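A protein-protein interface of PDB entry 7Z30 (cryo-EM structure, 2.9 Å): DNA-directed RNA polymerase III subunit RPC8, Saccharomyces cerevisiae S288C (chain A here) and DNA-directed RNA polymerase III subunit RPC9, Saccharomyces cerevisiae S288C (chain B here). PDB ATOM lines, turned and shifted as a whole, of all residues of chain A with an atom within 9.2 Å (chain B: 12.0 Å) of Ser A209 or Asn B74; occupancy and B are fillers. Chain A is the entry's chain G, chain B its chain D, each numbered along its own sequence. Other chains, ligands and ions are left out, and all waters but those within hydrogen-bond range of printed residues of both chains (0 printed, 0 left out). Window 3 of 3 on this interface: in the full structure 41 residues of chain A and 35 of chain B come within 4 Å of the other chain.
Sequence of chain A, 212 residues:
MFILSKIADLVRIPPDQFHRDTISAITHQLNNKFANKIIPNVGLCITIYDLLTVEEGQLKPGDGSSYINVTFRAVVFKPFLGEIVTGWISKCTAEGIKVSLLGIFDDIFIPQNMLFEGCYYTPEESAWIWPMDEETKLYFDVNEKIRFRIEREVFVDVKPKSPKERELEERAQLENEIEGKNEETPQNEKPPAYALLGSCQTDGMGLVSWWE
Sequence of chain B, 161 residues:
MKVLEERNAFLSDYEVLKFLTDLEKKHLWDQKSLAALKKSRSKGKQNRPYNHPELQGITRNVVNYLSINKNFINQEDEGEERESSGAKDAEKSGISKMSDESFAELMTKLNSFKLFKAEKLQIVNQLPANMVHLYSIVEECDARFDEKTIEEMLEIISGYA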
ATOM      1  N   LEU A 138      -8.083  16.848  -4.843  1.00  0.00           N
ATOM      2  CA  LEU A 138      -7.637  17.610  -5.999  1.00  0.00           C
ATOM      3  C   LEU A 138      -8.825  18.371  -6.581  1.00  0.00           C
ATOM      4  O   LEU A 138      -9.976  17.951  -6.428  1.00  0.00           O
ATOM      5  CB  LEU A 138      -7.000  16.655  -7.034  1.00  0.00           C
ATOM      6  CG  LEU A 138      -6.066  17.092  -8.171  1.00  0.00           C
ATOM      7  CD1 LEU A 138      -6.766  17.814  -9.305  1.00  0.00           C
ATOM      8  CD2 LEU A 138      -4.955  17.961  -7.597  1.00  0.00           C
ATOM      9  N   TYR A 139      -8.544  19.489  -7.251  1.00  0.00           N
ATOM     10  CA  TYR A 139      -9.603  20.331  -7.803  1.00  0.00           C
ATOM     11  C   TYR A 139      -9.100  20.988  -9.085  1.00  0.00           C
ATOM     12  O   TYR A 139      -8.065  20.605  -9.637  1.00  0.00           O
ATOM     13  CB  TYR A 139     -10.068  21.374  -6.780  1.00  0.00           C
ATOM     14  CG  TYR A 139      -8.956  22.198  -6.168  1.00  0.00           C
ATOM     15  CD1 TYR A 139      -8.295  21.773  -5.021  1.00  0.00           C
ATOM     16  CD2 TYR A 139      -8.575  23.408  -6.733  1.00  0.00           C
ATOM     17  CE1 TYR A 139      -7.278  22.531  -4.460  1.00  0.00           C
ATOM     18  CE2 TYR A 139      -7.563  24.170  -6.181  1.00  0.00           C
ATOM     19  CZ  TYR A 139      -6.918  23.728  -5.045  1.00  0.00           C
ATOM     20  OH  TYR A 139      -5.913  24.488  -4.498  1.00  0.00           O
ATOM     21  N   PHE A 140      -9.836  21.991  -9.561  1.00  0.00           N
ATOM     22  CA  PHE A 140      -9.503  22.652 -10.817  1.00  0.00           C
ATOM     23  C   PHE A 140      -9.900  24.119 -10.743  1.00  0.00           C
ATOM     24  O   PHE A 140     -10.668  24.536  -9.871  1.00  0.00           O
ATOM     25  CB  PHE A 140     -10.199  21.987 -12.012  1.00  0.00           C
ATOM     26  CG  PHE A 140     -11.696  21.891 -11.878  1.00  0.00           C
ATOM     27  CD1 PHE A 140     -12.285  20.783 -11.289  1.00  0.00           C
ATOM     28  CD2 PHE A 140     -12.514  22.906 -12.348  1.00  0.00           C
ATOM     29  CE1 PHE A 140     -13.660  20.693 -11.170  1.00  0.00           C
ATOM     30  CE2 PHE A 140     -13.889  22.821 -12.231  1.00  0.00           C
ATOM     31  CZ  PHE A 140     -14.463  21.713 -11.642  1.00  0.00           C
ATOM     32  N   GLU A 144     -10.419  25.545 -18.209  1.00  0.00           N
ATOM     33  CA  GLU A 144      -9.656  24.308 -18.311  1.00  0.00           C
ATOM     34  C   GLU A 144     -10.586  23.232 -18.853  1.00  0.00           C
ATOM     35  O   GLU A 144     -11.809  23.367 -18.806  1.00  0.00           O
ATOM     36  CB  GLU A 144      -9.056  23.907 -16.957  1.00  0.00           C
ATOM     37  CG  GLU A 144      -7.986  22.805 -16.994  1.00  0.00           C
ATOM     38  CD  GLU A 144      -6.697  23.212 -17.699  1.00  0.00           C
ATOM     39  OE1 GLU A 144      -6.747  23.737 -18.832  1.00  0.00           O
ATOM     40  OE2 GLU A 144      -5.616  23.000 -17.110  1.00  0.00           O
ATOM     41  N   LYS A 145      -9.988  22.165 -19.379  1.00  0.00           N
ATOM     42  CA  LYS A 145     -10.756  21.067 -19.947  1.00  0.00           C
ATOM     43  C   LYS A 145     -11.677  20.447 -18.899  1.00  0.00           C
ATOM     44  O   LYS A 145     -11.312  20.268 -17.734  1.00  0.00           O
ATOM     45  CB  LYS A 145      -9.821  19.998 -20.513  1.00  0.00           C
ATOM     46  CG  LYS A 145      -9.722  19.972 -22.033  1.00  0.00           C
ATOM     47  CD  LYS A 145      -9.709  21.374 -22.620  1.00  0.00           C
ATOM     48  CE  LYS A 145      -8.377  22.068 -22.376  1.00  0.00           C
ATOM     49  NZ  LYS A 145      -8.293  23.372 -23.086  1.00  0.00           N
ATOM     50  N   ILE A 146     -12.892  20.113 -19.331  1.00  0.00           N
ATOM     51  CA  ILE A 146     -13.884  19.456 -18.490  1.00  0.00           C
ATOM     52  C   ILE A 146     -14.344  18.205 -19.225  1.00  0.00           C
ATOM     53  O   ILE A 146     -14.196  18.080 -20.441  1.00  0.00           O
ATOM     54  CB  ILE A 146     -15.103  20.355 -18.163  1.00  0.00           C
ATOM     55  CG1 ILE A 146     -14.680  21.790 -17.871  1.00  0.00           C
ATOM     56  CG2 ILE A 146     -15.884  19.815 -16.971  1.00  0.00           C
ATOM     57  CD1 ILE A 146     -14.754  22.669 -19.083  1.00  0.00           C
ATOM     58  N   ARG A 147     -14.904  17.264 -18.471  1.00  0.00           N
ATOM     59  CA  ARG A 147     -15.482  16.062 -19.043  1.00  0.00           C
ATOM     60  C   ARG A 147     -16.752  15.741 -18.272  1.00  0.00           C
ATOM     61  O   ARG A 147     -16.734  15.678 -17.040  1.00  0.00           O
ATOM     62  CB  ARG A 147     -14.494  14.896 -18.991  1.00  0.00           C
ATOM     63  CG  ARG A 147     -14.750  13.837 -20.027  1.00  0.00           C
ATOM     64  CD  ARG A 147     -13.510  13.012 -20.315  1.00  0.00           C
ATOM     65  NE  ARG A 147     -13.327  11.929 -19.357  1.00  0.00           N
ATOM     66  CZ  ARG A 147     -12.227  11.739 -18.643  1.00  0.00           C
ATOM     67  NH1 ARG A 147     -11.193  12.558 -18.732  1.00  0.00           N
ATOM     68  NH2 ARG A 147     -12.155  10.689 -17.830  1.00  0.00           N
ATOM     69  N   GLY A 204     -12.777  10.116 -13.281  1.00  0.00           N
ATOM     70  CA  GLY A 204     -12.232  10.527 -14.547  1.00  0.00           C
ATOM     71  C   GLY A 204     -12.834  11.799 -15.115  1.00  0.00           C
ATOM     72  O   GLY A 204     -12.108  12.785 -15.283  1.00  0.00           O
ATOM     73  N   MET A 205     -14.133  11.812 -15.406  1.00  0.00           N
ATOM     74  CA  MET A 205     -14.717  12.961 -16.087  1.00  0.00           C
ATOM     75  C   MET A 205     -14.701  14.192 -15.187  1.00  0.00           C
ATOM     76  O   MET A 205     -14.880  14.108 -13.971  1.00  0.00           O
ATOM     77  CB  MET A 205     -16.143  12.675 -16.558  1.00  0.00           C
ATOM     78  CG  MET A 205     -17.076  12.043 -15.566  1.00  0.00           C
ATOM     79  SD  MET A 205     -18.201  10.967 -16.472  1.00  0.00           S
ATOM     80  CE  MET A 205     -19.358  10.553 -15.183  1.00  0.00           C
ATOM     81  N   GLY A 206     -14.490  15.351 -15.813  1.00  0.00           N
ATOM     82  CA  GLY A 206     -14.134  16.581 -15.140  1.00  0.00           C
ATOM     83  C   GLY A 206     -12.786  17.116 -15.578  1.00  0.00           C
ATOM     84  O   GLY A 206     -12.572  18.335 -15.557  1.00  0.00           O
ATOM     85  N   LEU A 207     -11.882  16.228 -15.984  1.00  0.00           N
ATOM     86  CA  LEU A 207     -10.593  16.592 -16.554  1.00  0.00           C
ATOM     87  C   LEU A 207     -10.067  15.395 -17.329  1.00  0.00           C
ATOM     88  O   LEU A 207     -10.330  14.243 -16.971  1.00  0.00           O
ATOM     89  CB  LEU A 207      -9.588  17.020 -15.479  1.00  0.00           C
ATOM     90  CG  LEU A 207      -8.227  17.526 -15.971  1.00  0.00           C
ATOM     91  CD1 LEU A 207      -8.371  18.805 -16.796  1.00  0.00           C
ATOM     92  CD2 LEU A 207      -7.263  17.730 -14.808  1.00  0.00           C
ATOM     93  N   VAL A 208      -9.326  15.680 -18.402  1.00  0.00           N
ATOM     94  CA  VAL A 208      -8.710  14.640 -19.216  1.00  0.00           C
ATOM     95  C   VAL A 208      -7.297  14.306 -18.764  1.00  0.00           C
ATOM     96  O   VAL A 208      -6.624  13.494 -19.414  1.00  0.00           O
ATOM     97  CB  VAL A 208      -8.715  15.034 -20.708  1.00  0.00           C
ATOM     98  CG1 VAL A 208     -10.143  15.233 -21.197  1.00  0.00           C
ATOM     99  CG2 VAL A 208      -7.887  16.295 -20.928  1.00  0.00           C
ATOM    100  N   SER A 209      -6.824  14.907 -17.672  1.00  0.00           N
ATOM    101  CA  SER A 209      -5.458  14.702 -17.202  1.00  0.00           C
ATOM    102  C   SER A 209      -5.421  14.541 -15.688  1.00  0.00           C
ATOM    103  O   SER A 209      -4.616  15.179 -15.001  1.00  0.00           O
ATOM    104  CB  SER A 209      -4.551  15.852 -17.635  1.00  0.00           C
ATOM    105  OG  SER A 209      -5.248  17.085 -17.618  1.00  0.00           O
ATOM    106  N   TRP A 210      -6.292  13.691 -15.140  1.00  0.00           N
ATOM    107  CA  TRP A 210      -6.278  13.479 -13.696  1.00  0.00           C
ATOM    108  C   TRP A 210      -5.100  12.618 -13.254  1.00  0.00           C
ATOM    109  O   TRP A 210      -4.601  12.787 -12.137  1.00  0.00           O
ATOM    110  CB  TRP A 210      -7.600  12.867 -13.230  1.00  0.00           C
ATOM    111  CG  TRP A 210      -8.597  13.897 -12.785  1.00  0.00           C
ATOM    112  CD1 TRP A 210      -8.412  15.248 -12.743  1.00  0.00           C
ATOM    113  CD2 TRP A 210      -9.922  13.661 -12.291  1.00  0.00           C
ATOM    114  NE1 TRP A 210      -9.541  15.869 -12.269  1.00  0.00           N
ATOM    115  CE2 TRP A 210     -10.483  14.916 -11.982  1.00  0.00           C
ATOM    116  CE3 TRP A 210     -10.690  12.510 -12.085  1.00  0.00           C
ATOM    117  CZ2 TRP A 210     -11.775  15.054 -11.480  1.00  0.00           C
ATOM    118  CZ3 TRP A 210     -11.974  12.650 -11.585  1.00  0.00           C
ATOM    119  CH2 TRP A 210     -12.502  13.912 -11.289  1.00  0.00           C
ATOM    120  N   TRP A 211      -4.642  11.696 -14.100  1.00  0.00           N
ATOM    121  CA  TRP A 211      -3.498  10.857 -13.772  1.00  0.00           C
ATOM    122  C   TRP A 211      -2.641  10.656 -15.014  1.00  0.00           C
ATOM    123  O   TRP A 211      -3.000  11.070 -16.120  1.00  0.00           O
ATOM    124  CB  TRP A 211      -3.928   9.501 -13.194  1.00  0.00           C
ATOM    125  CG  TRP A 211      -4.889   9.604 -12.049  1.00  0.00           C
ATOM    126  CD1 TRP A 211      -4.577   9.750 -10.728  1.00  0.00           C
ATOM    127  CD2 TRP A 211      -6.318   9.542 -12.120  1.00  0.00           C
ATOM    128  NE1 TRP A 211      -5.726   9.800  -9.975  1.00  0.00           N
ATOM    129  CE2 TRP A 211      -6.808   9.671 -10.805  1.00  0.00           C
ATOM    130  CE3 TRP A 211      -7.232   9.393 -13.168  1.00  0.00           C
ATOM    131  CZ2 TRP A 211      -8.169   9.657 -10.510  1.00  0.00           C
ATOM    132  CZ3 TRP A 211      -8.585   9.381 -12.873  1.00  0.00           C
ATOM    133  CH2 TRP A 211      -9.039   9.512 -11.556  1.00  0.00           C
ATOM    134  N   GLU A 212      -1.494  10.010 -14.810  1.00  0.00           N
ATOM    135  CA  GLU A 212      -0.529   9.725 -15.873  1.00  0.00           C
ATOM    136  C   GLU A 212      -0.064  10.997 -16.575  1.00  0.00           C
ATOM    137  O   GLU A 212       1.074  11.434 -16.400  1.00  0.00           O
ATOM    138  CB  GLU A 212      -1.119   8.744 -16.891  1.00  0.00           C
ATOM    139  CG  GLU A 212      -1.561   7.421 -16.290  1.00  0.00           C
ATOM    140  CD  GLU A 212      -3.050   7.375 -16.009  1.00  0.00           C
ATOM    141  OE1 GLU A 212      -3.782   8.248 -16.518  1.00  0.00           O
ATOM    142  OE2 GLU A 212      -3.487   6.467 -15.271  1.00  0.00           O
ATOM    143  N   SER B  67     -10.244  20.178 -34.951  1.00  0.00           N
ATOM    144  CA  SER B  67      -8.823  20.249 -35.267  1.00  0.00           C
ATOM    145  C   SER B  67      -7.952  20.372 -34.026  1.00  0.00           C
ATOM    146  O   SER B  67      -6.739  20.156 -34.115  1.00  0.00           O
ATOM    147  CB  SER B  67      -8.554  21.425 -36.207  1.00  0.00           C
ATOM    148  OG  SER B  67      -8.434  22.639 -35.486  1.00  0.00           O
ATOM    149  N   ILE B  68      -8.527  20.734 -32.880  1.00  0.00           N
ATOM    150  CA  ILE B  68      -7.733  20.748 -31.657  1.00  0.00           C
ATOM    151  C   ILE B  68      -7.329  19.320 -31.303  1.00  0.00           C
ATOM    152  O   ILE B  68      -8.036  18.350 -31.609  1.00  0.00           O
ATOM    153  CB  ILE B  68      -8.492  21.424 -30.501  1.00  0.00           C
ATOM    154  CG1 ILE B  68      -7.499  21.995 -29.492  1.00  0.00           C
ATOM    155  CG2 ILE B  68      -9.426  20.444 -29.810  1.00  0.00           C
ATOM    156  CD1 ILE B  68      -7.979  23.246 -28.812  1.00  0.00           C
ATOM    157  N   ASN B  69      -6.157  19.186 -30.683  1.00  0.00           N
ATOM    158  CA  ASN B  69      -5.620  17.867 -30.370  1.00  0.00           C
ATOM    159  C   ASN B  69      -6.565  17.100 -29.453  1.00  0.00           C
ATOM    160  O   ASN B  69      -7.077  17.640 -28.468  1.00  0.00           O
ATOM    161  CB  ASN B  69      -4.239  17.995 -29.723  1.00  0.00           C
ATOM    162  CG  ASN B  69      -4.195  19.054 -28.637  1.00  0.00           C
ATOM    163  OD1 ASN B  69      -5.165  19.779 -28.420  1.00  0.00           O
ATOM    164  ND2 ASN B  69      -3.065  19.145 -27.947  1.00  0.00           N
ATOM    165  N   LYS B  70      -6.802  15.833 -29.793  1.00  0.00           N
ATOM    166  CA  LYS B  70      -7.727  15.016 -29.019  1.00  0.00           C
ATOM    167  C   LYS B  70      -7.213  14.851 -27.596  1.00  0.00           C
ATOM    168  O   LYS B  70      -6.022  14.621 -27.369  1.00  0.00           O
ATOM    169  CB  LYS B  70      -7.916  13.648 -29.675  1.00  0.00           C
ATOM    170  CG  LYS B  70      -8.730  13.674 -30.963  1.00  0.00           C
ATOM    171  CD  LYS B  70      -8.982  12.271 -31.506  1.00  0.00           C
ATOM    172  CE  LYS B  70      -7.741  11.392 -31.483  1.00  0.00           C
ATOM    173  NZ  LYS B  70      -6.547  12.043 -32.082  1.00  0.00           N
ATOM    174  N   ASN B  71      -8.121  14.975 -26.632  1.00  0.00           N
ATOM    175  CA  ASN B  71      -7.743  15.074 -25.222  1.00  0.00           C
ATOM    176  C   ASN B  71      -7.618  13.692 -24.574  1.00  0.00           C
ATOM    177  O   ASN B  71      -8.241  13.388 -23.558  1.00  0.00           O
ATOM    178  CB  ASN B  71      -8.741  15.950 -24.475  1.00  0.00           C
ATOM    179  CG  ASN B  71      -8.765  17.373 -24.990  1.00  0.00           C
ATOM    180  OD1 ASN B  71      -7.736  18.050 -25.024  1.00  0.00           O
ATOM    181  ND2 ASN B  71      -9.941  17.838 -25.398  1.00  0.00           N
ATOM    182  N   PHE B  72      -6.786  12.844 -25.184  1.00  0.00           N
ATOM    183  CA  PHE B  72      -6.318  11.663 -24.470  1.00  0.00           C
ATOM    184  C   PHE B  72      -5.349  12.044 -23.360  1.00  0.00           C
ATOM    185  O   PHE B  72      -5.305  11.370 -22.326  1.00  0.00           O
ATOM    186  CB  PHE B  72      -5.649  10.670 -25.426  1.00  0.00           C
ATOM    187  CG  PHE B  72      -4.401  11.195 -26.080  1.00  0.00           C
ATOM    188  CD1 PHE B  72      -4.474  11.985 -27.214  1.00  0.00           C
ATOM    189  CD2 PHE B  72      -3.152  10.892 -25.562  1.00  0.00           C
ATOM    190  CE1 PHE B  72      -3.327  12.467 -27.818  1.00  0.00           C
ATOM    191  CE2 PHE B  72      -2.001  11.369 -26.161  1.00  0.00           C
ATOM    192  CZ  PHE B  72      -2.089  12.158 -27.290  1.00  0.00           C
ATOM    193  N   ILE B  73      -4.578  13.112 -23.561  1.00  0.00           N
ATOM    194  CA  ILE B  73      -3.661  13.624 -22.551  1.00  0.00           C
ATOM    195  C   ILE B  73      -3.800  15.138 -22.545  1.00  0.00           C
ATOM    196  O   ILE B  73      -4.424  15.724 -23.433  1.00  0.00           O
ATOM    197  CB  ILE B  73      -2.202  13.184 -22.839  1.00  0.00           C
ATOM    198  CG1 ILE B  73      -1.388  13.125 -21.545  1.00  0.00           C
ATOM    199  CG2 ILE B  73      -1.552  14.115 -23.851  1.00  0.00           C
ATOM    200  CD1 ILE B  73      -1.823  12.027 -20.601  1.00  0.00           C
ATOM    201  N   ASN B  74      -3.227  15.778 -21.532  1.00  0.00           N
ATOM    202  CA  ASN B  74      -3.236  17.233 -21.448  1.00  0.00           C
ATOM    203  C   ASN B  74      -2.362  17.854 -22.534  1.00  0.00           C
ATOM    204  O   ASN B  74      -2.857  18.269 -23.582  1.00  0.00           O
ATOM    205  CB  ASN B  74      -2.768  17.691 -20.067  1.00  0.00           C
ATOM    206  CG  ASN B  74      -1.499  16.993 -19.620  1.00  0.00           C
ATOM    207  OD1 ASN B  74      -0.850  16.298 -20.403  1.00  0.00           O
ATOM    208  ND2 ASN B  74      -1.141  17.171 -18.354  1.00  0.00           N
ATOM    209  N   GLU B  91       0.311  15.355 -31.336  1.00  0.00           N
ATOM    210  CA  GLU B  91       1.111  16.298 -32.108  1.00  0.00           C
ATOM    211  C   GLU B  91       0.303  16.840 -33.285  1.00  0.00           C
ATOM    212  O   GLU B  91       0.489  17.982 -33.707  1.00  0.00           O
ATOM    213  CB  GLU B  91       2.398  15.628 -32.601  1.00  0.00           C
ATOM    214  CG  GLU B  91       3.259  16.491 -33.514  1.00  0.00           C
ATOM    215  CD  GLU B  91       3.511  17.876 -32.947  1.00  0.00           C
ATOM    216  OE1 GLU B  91       3.911  17.973 -31.767  1.00  0.00           O
ATOM    217  OE2 GLU B  91       3.305  18.865 -33.681  1.00  0.00           O
ATOM    218  N   LYS B  92      -0.605  16.015 -33.800  1.00  0.00           N
ATOM    219  CA  LYS B  92      -1.415  16.407 -34.944  1.00  0.00           C
ATOM    220  C   LYS B  92      -2.713  17.068 -34.487  1.00  0.00           C
ATOM    221  O   LYS B  92      -2.914  17.366 -33.306  1.00  0.00           O
ATOM    222  CB  LYS B  92      -1.753  15.197 -35.822  1.00  0.00           C
ATOM    223  CG  LYS B  92      -0.596  14.267 -36.191  1.00  0.00           C
ATOM    224  CD  LYS B  92       0.729  14.993 -36.384  1.00  0.00           C
ATOM    225  CE  LYS B  92       1.889  14.011 -36.376  1.00  0.00           C
ATOM    226  NZ  LYS B  92       2.101  13.404 -35.034  1.00  0.00           N
ATOM    227  N   SER B  93      -3.603  17.299 -35.454  1.00  0.00           N
ATOM    228  CA  SER B  93      -4.952  17.737 -35.127  1.00  0.00           C
ATOM    229  C   SER B  93      -5.768  16.615 -34.502  1.00  0.00           C
ATOM    230  O   SER B  93      -6.590  16.874 -33.617  1.00  0.00           O
ATOM    231  CB  SER B  93      -5.659  18.262 -36.378  1.00  0.00           C
ATOM    232  OG  SER B  93      -6.526  17.280 -36.919  1.00  0.00           O
ATOM    233  N   LEU B 127     -11.551  10.154 -26.217  1.00  0.00           N
ATOM    234  CA  LEU B 127     -11.259   9.286 -25.080  1.00  0.00           C
ATOM    235  C   LEU B 127     -10.558   7.983 -25.455  1.00  0.00           C
ATOM    236  O   LEU B 127     -11.121   6.900 -25.253  1.00  0.00           O
ATOM    237  CB  LEU B 127     -12.551   8.979 -24.324  1.00  0.00           C
ATOM    238  CG  LEU B 127     -13.253  10.169 -23.666  1.00  0.00           C
ATOM    239  CD1 LEU B 127     -14.056   9.699 -22.472  1.00  0.00           C
ATOM    240  CD2 LEU B 127     -12.254  11.241 -23.248  1.00  0.00           C
ATOM    241  N   PRO B 128      -9.334   8.035 -25.997  1.00  0.00           N
ATOM    242  CA  PRO B 128      -8.556   6.802 -26.160  1.00  0.00           C
ATOM    243  C   PRO B 128      -7.574   6.581 -25.017  1.00  0.00           C
ATOM    244  O   PRO B 128      -7.385   7.463 -24.173  1.00  0.00           O
ATOM    245  CB  PRO B 128      -7.827   7.022 -27.491  1.00  0.00           C
ATOM    246  CG  PRO B 128      -7.802   8.525 -27.692  1.00  0.00           C
ATOM    247  CD  PRO B 128      -8.676   9.178 -26.653  1.00  0.00           C
ATOM    248  N   ALA B 129      -6.948   5.401 -24.988  1.00  0.00           N
ATOM    249  CA  ALA B 129      -5.868   5.058 -24.064  1.00  0.00           C
ATOM    250  C   ALA B 129      -6.257   5.201 -22.596  1.00  0.00           C
ATOM    251  O   ALA B 129      -5.429   5.613 -21.776  1.00  0.00           O
ATOM    252  CB  ALA B 129      -4.612   5.890 -24.347  1.00  0.00           C
ATOM    253  N   ASN B 130      -7.497   4.877 -22.236  1.00  0.00           N
ATOM    254  CA  ASN B 130      -7.918   4.938 -20.844  1.00  0.00           C
ATOM    255  C   ASN B 130      -9.094   3.997 -20.635  1.00  0.00           C
ATOM    256  O   ASN B 130     -10.113   4.105 -21.322  1.00  0.00           O
ATOM    257  CB  ASN B 130      -8.294   6.368 -20.439  1.00  0.00           C
ATOM    258  CG  ASN B 130      -8.541   6.507 -18.949  1.00  0.00           C
ATOM    259  OD1 ASN B 130      -7.669   6.211 -18.134  1.00  0.00           O
ATOM    260  ND2 ASN B 130      -9.729   6.973 -18.589  1.00  0.00           N
ATOM    261  N   VAL B 132     -11.023   3.787 -17.933  1.00  0.00           N
ATOM    262  CA  VAL B 132     -12.151   4.522 -17.372  1.00  0.00           C
ATOM    263  C   VAL B 132     -12.931   5.223 -18.474  1.00  0.00           C
ATOM    264  O   VAL B 132     -14.164   5.311 -18.415  1.00  0.00           O
ATOM    265  CB  VAL B 132     -11.666   5.522 -16.305  1.00  0.00           C
ATOM    266  CG1 VAL B 132     -12.805   5.897 -15.371  1.00  0.00           C
ATOM    267  CG2 VAL B 132     -10.495   4.942 -15.525  1.00  0.00           C
ATOM    268  N   HIS B 133     -12.230   5.737 -19.488  1.00  0.00           N
ATOM    269  CA  HIS B 133     -12.896   6.342 -20.636  1.00  0.00           C
ATOM    270  C   HIS B 133     -13.873   5.365 -21.275  1.00  0.00           C
ATOM    271  O   HIS B 133     -15.049   5.683 -21.478  1.00  0.00           O
ATOM    272  CB  HIS B 133     -11.854   6.794 -21.659  1.00  0.00           C
ATOM    273  CG  HIS B 133     -11.176   8.082 -21.313  1.00  0.00           C
ATOM    274  ND1 HIS B 133     -10.095   8.564 -22.020  1.00  0.00           N
ATOM    275  CD2 HIS B 133     -11.423   8.989 -20.339  1.00  0.00           C
ATOM    276  CE1 HIS B 133      -9.703   9.710 -21.494  1.00  0.00           C
ATOM    277  NE2 HIS B 133     -10.493   9.992 -20.475  1.00  0.00           N
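A ring nitrogen (NE2) of His B133 lies close to the guanidinium group (NH1) of Arg A147, at 3.2 Å.
NH2 of Arg A147 lies close to O of Gly A204 (3.3 Å).
NH1 of Arg A147 sits at hydrogen-bond distance from O of Leu A207.
The backbone carbonyl oxygen (O) of Arg A147 sits at hydrogen-bond distance from the backbone NH (N) of Gly A206.
The backbone NH of His B133 lies close to the side-chain amide nitrogen of Asn B130 (2.9 Å).
Lys A145 touches Asn B71.
CD2 of Leu B127 touches CD of Arg A147, 3.6 Å away.
CB of Val A208 touches O of Asn B71 (3.3 Å).
Val A208 touches Phe B72.
CB of Ser A209 touches CB of Asn B74, 3.5 Å away.
Printed residues of chain B within 4 Å of Lys A145: Asn B71.
Of the printed residues of chain B, Arg A147 touches Leu B127 and His B133.
No residue of chain B comes within 4 Å of Gly A206.
Leu A207 touches none of the printed residues of chain B.
Of chain B, only Asn B74 (3.5 Å) comes within 4 Å of Ser A209.
Trp A211 touches none of the printed residues of chain B.
Of the printed residues of chain A, Asn B71 touches Lys A145 (3.99 Å) and Val A208 (3.3 Å).
No residue of chain A comes within 4 Å of Ile B73.
Printed residues of chain A within 4 Å of Asn B74: Ser A209.
Of the printed residues of chain A, Leu B127 touches Arg A147.
Of the printed residues of chain A, His B133 touches Arg A147.
The nearest residue of chain B that does not touch Ser A209 is Ile B73 (5.0 Å).
The nearest printed residue of chain A that does not touch Asn B71 is Arg A147 (5.7 Å).
Hydrophobic or aromatic side chains of chain A within 4 Å of the printed part of chain B: Val A208.
Among the printed residues, 6 pairs touch across the chains.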
